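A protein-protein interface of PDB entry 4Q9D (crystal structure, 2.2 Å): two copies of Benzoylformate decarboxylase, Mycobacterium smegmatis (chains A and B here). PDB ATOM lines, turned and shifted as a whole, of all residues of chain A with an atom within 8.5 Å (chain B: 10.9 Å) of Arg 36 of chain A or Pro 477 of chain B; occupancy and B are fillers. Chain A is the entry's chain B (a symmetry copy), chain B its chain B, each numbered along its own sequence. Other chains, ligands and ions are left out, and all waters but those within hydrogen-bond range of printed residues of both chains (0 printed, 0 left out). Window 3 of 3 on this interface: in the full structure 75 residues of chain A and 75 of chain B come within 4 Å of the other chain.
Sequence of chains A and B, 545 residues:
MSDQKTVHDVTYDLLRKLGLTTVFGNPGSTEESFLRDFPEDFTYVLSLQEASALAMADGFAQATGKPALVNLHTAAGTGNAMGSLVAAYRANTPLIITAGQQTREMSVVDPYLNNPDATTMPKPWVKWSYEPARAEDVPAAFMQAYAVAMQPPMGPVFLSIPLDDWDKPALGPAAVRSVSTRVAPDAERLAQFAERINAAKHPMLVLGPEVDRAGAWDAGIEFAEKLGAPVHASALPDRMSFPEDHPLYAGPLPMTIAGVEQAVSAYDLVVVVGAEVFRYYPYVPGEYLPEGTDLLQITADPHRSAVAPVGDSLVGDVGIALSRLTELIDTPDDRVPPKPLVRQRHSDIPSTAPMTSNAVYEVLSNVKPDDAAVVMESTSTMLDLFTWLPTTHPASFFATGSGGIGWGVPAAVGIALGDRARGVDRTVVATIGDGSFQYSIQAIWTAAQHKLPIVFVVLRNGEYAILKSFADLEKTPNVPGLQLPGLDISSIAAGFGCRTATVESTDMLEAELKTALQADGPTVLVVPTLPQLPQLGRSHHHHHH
The backbone carbonyl oxygen (O) of Asn 478 of chain B sits at hydrogen-bond distance from the backbone NH (N) of Asp 37 of chain A (3.4 Å).
The backbone carbonyl oxygen (O) of Arg 36 of chain A is in hydrogen-bond range of a ring nitrogen (NE2) of His 8 of chain A, 2.9 Å away.
The side-chain carboxylate (OE2) of Glu 32 of chain A is in salt-bridge range of the guanidinium group (NH1) of Arg 36 of chain A, 3.6 Å away.
The guanidinium group (NH2) of Arg 36 of chain A is in salt-bridge range of the side-chain carboxylate (OD2) of Asp 167 of chain A (3.2 Å).
Among the printed residues, pairs that only touch across the chains: Glu 32 of chain A with Ile 466 of chain B, Glu 32 of chain A with Pro 477 of chain B, Glu 32 of chain A with Val 479 of chain B, Leu 35 of chain A with Asn 478 of chain B, Leu 35 of chain A with Pro 480 of chain B, Arg 36 of chain A with Pro 477 of chain B, Arg 36 of chain A with Val 479 of chain B, Phe 38 of chain A with Asn 478 of chain B and Phe 38 of chain A with Pro 480 of chain B.
Printed residues of chain B within 4 Å of Glu 32 of chain A: Ile 466, Pro 477 and Val 479.
No residue of chain B comes within 4 Å of Ser 33 of chain A.
Leu 35 of chain A touches two residues of chain B.
Asp 37 of chain A touches just one residue of chain B: Asn 478.
Printed residues of chain B within 4 Å of Phe 38 of chain A: Asn 478 (3.7 Å) and Pro 480 (3.8 Å).
Printed residues of chain A within 4 Å of Ile 466 of chain B: Glu 32 (3.6 Å).
Pro 477 of chain B touches just these residues of chain A: Glu 32 and Arg 36.
Printed residues of chain A within 4 Å of Asn 478 of chain B: Leu 35 (3.6 Å), Asp 37 (3.4 Å) and Phe 38 (3.7 Å).
Of the printed residues of chain A, Val 479 of chain B touches Glu 32 and Arg 36.
Printed residues of chain A within 4 Å of Pro 480 of chain B: Leu 35 (3.3 Å) and Phe 38 (3.8 Å).
Gln 483 of chain B touches none of the printed residues of chain A.
The nearest printed residue of chain A that does not touch Val 479 of chain B is Leu 35 of chain A (4.1 Å).
Of the 19 printed residues of chain A, 5 touch a printed residue of chain B.
Hydrophobic or aromatic side chains of chain A within 4 Å of the printed part of chain B: Leu 35 and Phe 38.
Along chain A the printed residues that touch a printed residue of chain B span positions 32 to 38.
Printed residues of chain B that touch a printed residue of chain A: Ile 466, Pro 477, Asn 478, Val 479 and Pro 480.
Among the printed residues, 10 pairs touch across the chains.
Among the printed residues, no Asp or Glu carboxylate lies within 4 Å of a Lys or Arg side-chain nitrogen of the other chain.
No position is printed for both chains.
Of the 10 pairs that touch across the chains among the printed residues, none has its exchanged pair printed and touching as well.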
ATOM      1  N   HIS A   8      25.901   4.220  24.960  1.00  0.00           N
ATOM      2  CA  HIS A   8      25.057   4.627  26.088  1.00  0.00           C
ATOM      3  C   HIS A   8      25.838   5.519  27.071  1.00  0.00           C
ATOM      4  O   HIS A   8      25.362   6.595  27.456  1.00  0.00           O
ATOM      5  CB  HIS A   8      24.522   3.358  26.779  1.00  0.00           C
ATOM      6  CG  HIS A   8      23.473   3.603  27.821  1.00  0.00           C
ATOM      7  ND1 HIS A   8      23.767   4.091  29.081  1.00  0.00           N
ATOM      8  CD2 HIS A   8      22.131   3.397  27.806  1.00  0.00           C
ATOM      9  CE1 HIS A   8      22.658   4.167  29.797  1.00  0.00           C
ATOM     10  NE2 HIS A   8      21.646   3.755  29.046  1.00  0.00           N
ATOM     11  N   ASP A   9      27.041   5.081  27.467  1.00  0.00           N
ATOM     12  CA  ASP A   9      27.879   5.863  28.391  1.00  0.00           C
ATOM     13  C   ASP A   9      28.146   7.266  27.884  1.00  0.00           C
ATOM     14  O   ASP A   9      27.927   8.262  28.591  1.00  0.00           O
ATOM     15  CB  ASP A   9      29.261   5.199  28.623  1.00  0.00           C
ATOM     16  CG  ASP A   9      29.164   3.858  29.343  1.00  0.00           C
ATOM     17  OD1 ASP A   9      28.293   3.707  30.225  1.00  0.00           O
ATOM     18  OD2 ASP A   9      29.956   2.950  29.006  1.00  0.00           O
ATOM     19  N   TYR A  12      24.841   9.741  27.378  1.00  0.00           N
ATOM     20  CA  TYR A  12      24.412  10.371  28.628  1.00  0.00           C
ATOM     21  C   TYR A  12      25.444  11.385  29.136  1.00  0.00           C
ATOM     22  O   TYR A  12      25.078  12.450  29.630  1.00  0.00           O
ATOM     23  CB  TYR A  12      24.128   9.307  29.678  1.00  0.00           C
ATOM     24  CG  TYR A  12      22.732   8.750  29.567  1.00  0.00           C
ATOM     25  CD1 TYR A  12      21.643   9.435  30.125  1.00  0.00           C
ATOM     26  CD2 TYR A  12      22.482   7.567  28.873  1.00  0.00           C
ATOM     27  CE1 TYR A  12      20.352   8.933  30.013  1.00  0.00           C
ATOM     28  CE2 TYR A  12      21.197   7.053  28.766  1.00  0.00           C
ATOM     29  CZ  TYR A  12      20.133   7.745  29.340  1.00  0.00           C
ATOM     30  OH  TYR A  12      18.848   7.244  29.265  1.00  0.00           O
ATOM     31  N   GLY A  28       8.807   1.850  26.860  1.00  0.00           N
ATOM     32  CA  GLY A  28       8.384   0.595  26.267  1.00  0.00           C
ATOM     33  C   GLY A  28       9.586  -0.279  25.960  1.00  0.00           C
ATOM     34  O   GLY A  28      10.738   0.146  26.139  1.00  0.00           O
ATOM     35  N   SER A  29       9.318  -1.478  25.454  1.00  0.00           N
ATOM     36  CA  SER A  29      10.353  -2.486  25.210  1.00  0.00           C
ATOM     37  C   SER A  29      11.481  -1.961  24.341  1.00  0.00           C
ATOM     38  O   SER A  29      12.660  -2.220  24.619  1.00  0.00           O
ATOM     39  CB  SER A  29       9.725  -3.707  24.514  1.00  0.00           C
ATOM     40  OG  SER A  29       8.928  -3.294  23.393  1.00  0.00           O
ATOM     41  N   GLU A  31      12.548   0.936  24.037  1.00  0.00           N
ATOM     42  CA  GLU A  31      13.318   1.994  24.707  1.00  0.00           C
ATOM     43  C   GLU A  31      14.096   1.466  25.936  1.00  0.00           C
ATOM     44  O   GLU A  31      14.876   2.206  26.539  1.00  0.00           O
ATOM     45  CB  GLU A  31      12.406   3.190  25.100  1.00  0.00           C
ATOM     46  CG  GLU A  31      11.697   3.856  23.875  1.00  0.00           C
ATOM     47  CD  GLU A  31      10.759   2.902  23.173  1.00  0.00           C
ATOM     48  OE1 GLU A  31       9.909   2.298  23.870  1.00  0.00           O
ATOM     49  OE2 GLU A  31      10.884   2.723  21.933  1.00  0.00           O
ATOM     50  N   GLU A  32      13.898   0.200  26.303  1.00  0.00           N
ATOM     51  CA  GLU A  32      14.593  -0.330  27.488  1.00  0.00           C
ATOM     52  C   GLU A  32      16.128  -0.186  27.440  1.00  0.00           C
ATOM     53  O   GLU A  32      16.765   0.201  28.431  1.00  0.00           O
ATOM     54  CB  GLU A  32      14.202  -1.779  27.775  1.00  0.00           C
ATOM     55  CG  GLU A  32      15.260  -2.506  28.597  1.00  0.00           C
ATOM     56  CD  GLU A  32      14.669  -3.491  29.585  1.00  0.00           C
ATOM     57  OE1 GLU A  32      13.506  -3.912  29.375  1.00  0.00           O
ATOM     58  OE2 GLU A  32      15.369  -3.838  30.571  1.00  0.00           O
ATOM     59  N   SER A  33      16.742  -0.428  26.293  1.00  0.00           N
ATOM     60  CA  SER A  33      18.200  -0.341  26.275  1.00  0.00           C
ATOM     61  C   SER A  33      18.682   1.091  26.408  1.00  0.00           C
ATOM     62  O   SER A  33      19.831   1.323  26.822  1.00  0.00           O
ATOM     63  CB  SER A  33      18.801  -1.008  25.028  1.00  0.00           C
ATOM     64  OG  SER A  33      18.320  -0.409  23.837  1.00  0.00           O
ATOM     65  N   PHE A  34      17.820   2.055  26.059  1.00  0.00           N
ATOM     66  CA  PHE A  34      18.163   3.476  26.242  1.00  0.00           C
ATOM     67  C   PHE A  34      18.063   3.875  27.722  1.00  0.00           C
ATOM     68  O   PHE A  34      18.918   4.586  28.251  1.00  0.00           O
ATOM     69  CB  PHE A  34      17.237   4.395  25.399  1.00  0.00           C
ATOM     70  CG  PHE A  34      17.366   5.866  25.745  1.00  0.00           C
ATOM     71  CD1 PHE A  34      18.599   6.507  25.676  1.00  0.00           C
ATOM     72  CD2 PHE A  34      16.262   6.603  26.160  1.00  0.00           C
ATOM     73  CE1 PHE A  34      18.729   7.860  25.991  1.00  0.00           C
ATOM     74  CE2 PHE A  34      16.380   7.969  26.480  1.00  0.00           C
ATOM     75  CZ  PHE A  34      17.624   8.594  26.399  1.00  0.00           C
ATOM     76  N   LEU A  35      16.981   3.430  28.363  1.00  0.00           N
ATOM     77  CA  LEU A  35      16.607   3.869  29.710  1.00  0.00           C
ATOM     78  C   LEU A  35      17.305   3.094  30.832  1.00  0.00           C
ATOM     79  O   LEU A  35      17.365   3.561  31.976  1.00  0.00           O
ATOM     80  CB  LEU A  35      15.092   3.755  29.878  1.00  0.00           C
ATOM     81  CG  LEU A  35      14.309   4.728  28.973  1.00  0.00           C
ATOM     82  CD1 LEU A  35      12.838   4.553  29.176  1.00  0.00           C
ATOM     83  CD2 LEU A  35      14.718   6.175  29.286  1.00  0.00           C
ATOM     84  N   ARG A  36      17.795   1.906  30.496  1.00  0.00           N
ATOM     85  CA  ARG A  36      18.528   1.051  31.432  1.00  0.00           C
ATOM     86  C   ARG A  36      19.726   1.800  32.046  1.00  0.00           C
ATOM     87  O   ARG A  36      20.404   2.561  31.356  1.00  0.00           O
ATOM     88  CB  ARG A  36      19.016  -0.200  30.689  1.00  0.00           C
ATOM     89  CG  ARG A  36      19.226  -1.422  31.572  1.00  0.00           C
ATOM     90  CD  ARG A  36      19.017  -2.727  30.795  1.00  0.00           C
ATOM     91  NE  ARG A  36      19.852  -2.809  29.592  1.00  0.00           N
ATOM     92  CZ  ARG A  36      19.445  -3.325  28.430  1.00  0.00           C
ATOM     93  NH1 ARG A  36      18.209  -3.801  28.307  1.00  0.00           N
ATOM     94  NH2 ARG A  36      20.266  -3.358  27.381  1.00  0.00           N
ATOM     95  N   ASP A  37      19.985   1.605  33.336  1.00  0.00           N
ATOM     96  CA  ASP A  37      21.094   2.303  33.992  1.00  0.00           C
ATOM     97  C   ASP A  37      20.981   3.805  33.831  1.00  0.00           C
ATOM     98  O   ASP A  37      21.974   4.486  33.597  1.00  0.00           O
ATOM     99  CB  ASP A  37      22.426   1.871  33.404  1.00  0.00           C
ATOM    100  CG  ASP A  37      22.826   0.501  33.859  1.00  0.00           C
ATOM    101  OD1 ASP A  37      22.584   0.217  35.048  1.00  0.00           O
ATOM    102  OD2 ASP A  37      23.348  -0.283  33.034  1.00  0.00           O
ATOM    103  N   PHE A  38      19.759   4.298  33.893  1.00  0.00           N
ATOM    104  CA  PHE A  38      19.504   5.723  33.800  1.00  0.00           C
ATOM    105  C   PHE A  38      20.362   6.393  34.886  1.00  0.00           C
ATOM    106  O   PHE A  38      20.269   6.007  36.047  1.00  0.00           O
ATOM    107  CB  PHE A  38      18.004   5.917  34.080  1.00  0.00           C
ATOM    108  CG  PHE A  38      17.464   7.266  33.721  1.00  0.00           C
ATOM    109  CD1 PHE A  38      17.335   7.653  32.380  1.00  0.00           C
ATOM    110  CD2 PHE A  38      17.003   8.121  34.719  1.00  0.00           C
ATOM    111  CE1 PHE A  38      16.793   8.895  32.043  1.00  0.00           C
ATOM    112  CE2 PHE A  38      16.434   9.362  34.394  1.00  0.00           C
ATOM    113  CZ  PHE A  38      16.333   9.751  33.057  1.00  0.00           C
ATOM    114  N   PRO A  39      21.177   7.411  34.528  1.00  0.00           N
ATOM    115  CA  PRO A  39      22.050   8.040  35.533  1.00  0.00           C
ATOM    116  C   PRO A  39      21.288   8.627  36.709  1.00  0.00           C
ATOM    117  O   PRO A  39      20.158   9.120  36.573  1.00  0.00           O
ATOM    118  CB  PRO A  39      22.736   9.161  34.755  1.00  0.00           C
ATOM    119  CG  PRO A  39      22.701   8.704  33.326  1.00  0.00           C
ATOM    120  CD  PRO A  39      21.346   8.040  33.204  1.00  0.00           C
ATOM    121  N   ASN A  71      11.095  10.938  25.205  1.00  0.00           N
ATOM    122  CA  ASN A  71      11.396   9.576  24.746  1.00  0.00           C
ATOM    123  C   ASN A  71      10.128   8.785  24.580  1.00  0.00           C
ATOM    124  O   ASN A  71       9.371   8.648  25.532  1.00  0.00           O
ATOM    125  CB  ASN A  71      12.388   8.875  25.709  1.00  0.00           C
ATOM    126  CG  ASN A  71      12.808   7.485  25.219  1.00  0.00           C
ATOM    127  OD1 ASN A  71      12.612   6.501  25.928  1.00  0.00           O
ATOM    128  ND2 ASN A  71      13.388   7.406  24.003  1.00  0.00           N
ATOM    129  N   LEU A 163      17.364  -0.206  18.914  1.00  0.00           N
ATOM    130  CA  LEU A 163      17.618  -0.524  20.319  1.00  0.00           C
ATOM    131  C   LEU A 163      18.994  -1.171  20.566  1.00  0.00           C
ATOM    132  O   LEU A 163      19.501  -1.145  21.685  1.00  0.00           O
ATOM    133  CB  LEU A 163      16.484  -1.395  20.873  1.00  0.00           C
ATOM    134  CG  LEU A 163      16.298  -2.797  20.258  1.00  0.00           C
ATOM    135  CD1 LEU A 163      17.194  -3.868  20.982  1.00  0.00           C
ATOM    136  CD2 LEU A 163      14.848  -3.174  20.377  1.00  0.00           C
ATOM    137  N   ASP A 164      19.612  -1.723  19.527  1.00  0.00           N
ATOM    138  CA  ASP A 164      20.871  -2.441  19.720  1.00  0.00           C
ATOM    139  C   ASP A 164      22.032  -1.480  19.708  1.00  0.00           C
ATOM    140  O   ASP A 164      23.143  -1.866  20.040  1.00  0.00           O
ATOM    141  CB  ASP A 164      21.060  -3.588  18.686  1.00  0.00           C
ATOM    142  CG  ASP A 164      20.904  -3.116  17.243  1.00  0.00           C
ATOM    143  OD1 ASP A 164      19.963  -2.348  16.964  1.00  0.00           O
ATOM    144  OD2 ASP A 164      21.709  -3.510  16.380  1.00  0.00           O
ATOM    145  N   TRP A 166      22.771   1.047  21.621  1.00  0.00           N
ATOM    146  CA  TRP A 166      23.185   1.655  22.882  1.00  0.00           C
ATOM    147  C   TRP A 166      24.328   0.881  23.547  1.00  0.00           C
ATOM    148  O   TRP A 166      25.154   1.460  24.240  1.00  0.00           O
ATOM    149  CB  TRP A 166      21.964   1.734  23.828  1.00  0.00           C
ATOM    150  CG  TRP A 166      20.956   2.762  23.340  1.00  0.00           C
ATOM    151  CD1 TRP A 166      19.759   2.520  22.740  1.00  0.00           C
ATOM    152  CD2 TRP A 166      21.122   4.188  23.348  1.00  0.00           C
ATOM    153  NE1 TRP A 166      19.149   3.705  22.404  1.00  0.00           N
ATOM    154  CE2 TRP A 166      19.964   4.744  22.765  1.00  0.00           C
ATOM    155  CE3 TRP A 166      22.130   5.044  23.806  1.00  0.00           C
ATOM    156  CZ2 TRP A 166      19.773   6.120  22.643  1.00  0.00           C
ATOM    157  CZ3 TRP A 166      21.950   6.416  23.665  1.00  0.00           C
ATOM    158  CH2 TRP A 166      20.777   6.939  23.080  1.00  0.00           C
ATOM    159  N   ASP A 167      24.352  -0.434  23.337  1.00  0.00           N
ATOM    160  CA  ASP A 167      25.371  -1.285  23.946  1.00  0.00           C
ATOM    161  C   ASP A 167      26.625  -1.437  23.101  1.00  0.00           C
ATOM    162  O   ASP A 167      27.549  -2.113  23.505  1.00  0.00           O
ATOM    163  CB  ASP A 167      24.781  -2.654  24.309  1.00  0.00           C
ATOM    164  CG  ASP A 167      23.783  -2.546  25.452  1.00  0.00           C
ATOM    165  OD1 ASP A 167      23.940  -1.582  26.257  1.00  0.00           O
ATOM    166  OD2 ASP A 167      22.847  -3.384  25.540  1.00  0.00           O
ATOM    167  N   PRO B 282      11.138  -9.827  20.623  1.00  0.00           N
ATOM    168  CA  PRO B 282      12.517  -9.728  21.140  1.00  0.00           C
ATOM    169  C   PRO B 282      13.507 -10.454  20.238  1.00  0.00           C
ATOM    170  O   PRO B 282      13.124 -11.355  19.471  1.00  0.00           O
ATOM    171  CB  PRO B 282      12.451 -10.421  22.500  1.00  0.00           C
ATOM    172  CG  PRO B 282      11.246 -11.348  22.423  1.00  0.00           C
ATOM    173  CD  PRO B 282      10.315 -10.803  21.371  1.00  0.00           C
ATOM    174  N   TYR B 283      14.766 -10.031  20.296  1.00  0.00           N
ATOM    175  CA  TYR B 283      15.798 -10.604  19.446  1.00  0.00           C
ATOM    176  C   TYR B 283      16.535 -11.740  20.165  1.00  0.00           C
ATOM    177  O   TYR B 283      17.179 -11.492  21.163  1.00  0.00           O
ATOM    178  CB  TYR B 283      16.809  -9.538  19.047  1.00  0.00           C
ATOM    179  CG  TYR B 283      17.851 -10.096  18.132  1.00  0.00           C
ATOM    180  CD1 TYR B 283      17.487 -10.589  16.891  1.00  0.00           C
ATOM    181  CD2 TYR B 283      19.203 -10.160  18.509  1.00  0.00           C
ATOM    182  CE1 TYR B 283      18.420 -11.105  16.015  1.00  0.00           C
ATOM    183  CE2 TYR B 283      20.151 -10.681  17.638  1.00  0.00           C
ATOM    184  CZ  TYR B 283      19.743 -11.155  16.382  1.00  0.00           C
ATOM    185  OH  TYR B 283      20.645 -11.694  15.493  1.00  0.00           O
ATOM    186  N   ILE B 466       6.871  -5.053  31.606  1.00  0.00           N
ATOM    187  CA  ILE B 466       8.171  -4.800  30.982  1.00  0.00           C
ATOM    188  C   ILE B 466       8.547  -5.856  29.928  1.00  0.00           C
ATOM    189  O   ILE B 466       8.307  -7.056  30.105  1.00  0.00           O
ATOM    190  CB  ILE B 466       9.283  -4.678  32.069  1.00  0.00           C
ATOM    191  CG1 ILE B 466      10.661  -4.442  31.438  1.00  0.00           C
ATOM    192  CG2 ILE B 466       9.278  -5.902  32.999  1.00  0.00           C
ATOM    193  CD1 ILE B 466      11.796  -4.328  32.460  1.00  0.00           C
ATOM    194  N   PRO B 477      17.020  -4.598  34.965  1.00  0.00           N
ATOM    195  CA  PRO B 477      18.083  -3.622  35.138  1.00  0.00           C
ATOM    196  C   PRO B 477      17.505  -2.377  35.819  1.00  0.00           C
ATOM    197  O   PRO B 477      16.563  -2.507  36.583  1.00  0.00           O
ATOM    198  CB  PRO B 477      18.520  -3.361  33.704  1.00  0.00           C
ATOM    199  CG  PRO B 477      17.371  -3.790  32.843  1.00  0.00           C
ATOM    200  CD  PRO B 477      16.299  -4.355  33.711  1.00  0.00           C
ATOM    201  N   ASN B 478      18.039  -1.194  35.588  1.00  0.00           N
ATOM    202  CA  ASN B 478      17.518  -0.082  36.382  1.00  0.00           C
ATOM    203  C   ASN B 478      16.716   0.928  35.545  1.00  0.00           C
ATOM    204  O   ASN B 478      17.205   2.036  35.259  1.00  0.00           O
ATOM    205  CB  ASN B 478      18.662   0.629  37.108  1.00  0.00           C
ATOM    206  CG  ASN B 478      18.446   0.688  38.599  1.00  0.00           C
ATOM    207  OD1 ASN B 478      17.709  -0.128  39.160  1.00  0.00           O
ATOM    208  ND2 ASN B 478      19.078   1.659  39.256  1.00  0.00           N
ATOM    209  N   VAL B 479      15.494   0.539  35.166  1.00  0.00           N
ATOM    210  CA  VAL B 479      14.672   1.311  34.228  1.00  0.00           C
ATOM    211  C   VAL B 479      13.642   2.179  34.956  1.00  0.00           C
ATOM    212  O   VAL B 479      12.826   1.665  35.715  1.00  0.00           O
ATOM    213  CB  VAL B 479      13.945   0.391  33.216  1.00  0.00           C
ATOM    214  CG1 VAL B 479      12.999   1.199  32.336  1.00  0.00           C
ATOM    215  CG2 VAL B 479      14.952  -0.364  32.350  1.00  0.00           C
ATOM    216  N   PRO B 480      13.691   3.498  34.723  1.00  0.00           N
ATOM    217  CA  PRO B 480      12.744   4.473  35.294  1.00  0.00           C
ATOM    218  C   PRO B 480      11.357   4.322  34.672  1.00  0.00           C
ATOM    219  O   PRO B 480      11.224   3.699  33.616  1.00  0.00           O
ATOM    220  CB  PRO B 480      13.341   5.821  34.886  1.00  0.00           C
ATOM    221  CG  PRO B 480      14.063   5.517  33.565  1.00  0.00           C
ATOM    222  CD  PRO B 480      14.626   4.118  33.764  1.00  0.00           C
ATOM    223  N   GLY B 481      10.337   4.839  35.346  1.00  0.00           N
ATOM    224  CA  GLY B 481       9.003   4.914  34.781  1.00  0.00           C
ATOM    225  C   GLY B 481       8.177   3.647  34.658  1.00  0.00           C
ATOM    226  O   GLY B 481       7.275   3.600  33.830  1.00  0.00           O
ATOM    227  N   LEU B 482       8.452   2.634  35.478  1.00  0.00           N
ATOM    228  CA  LEU B 482       7.683   1.391  35.408  1.00  0.00           C
ATOM    229  C   LEU B 482       6.533   1.304  36.414  1.00  0.00           C
ATOM    230  O   LEU B 482       5.605   0.520  36.223  1.00  0.00           O
ATOM    231  CB  LEU B 482       8.602   0.166  35.568  1.00  0.00           C
ATOM    232  CG  LEU B 482       9.654   0.037  34.460  1.00  0.00           C
ATOM    233  CD1 LEU B 482      10.484  -1.235  34.632  1.00  0.00           C
ATOM    234  CD2 LEU B 482       9.021   0.110  33.071  1.00  0.00           C
ATOM    235  N   GLN B 483       6.602   2.098  37.479  1.00  0.00           N
ATOM    236  CA  GLN B 483       5.661   1.979  38.595  1.00  0.00           C
ATOM    237  C   GLN B 483       4.461   2.899  38.382  1.00  0.00           C
ATOM    238  O   GLN B 483       4.629   4.000  37.874  1.00  0.00           O
ATOM    239  CB  GLN B 483       6.379   2.372  39.896  1.00  0.00           C
ATOM    240  CG  GLN B 483       7.597   1.478  40.230  1.00  0.00           C
ATOM    241  CD  GLN B 483       7.206   0.009  40.347  1.00  0.00           C
ATOM    242  OE1 GLN B 483       6.232  -0.334  41.030  1.00  0.00           O
ATOM    243  NE2 GLN B 483       7.951  -0.864  39.671  1.00  0.00           N
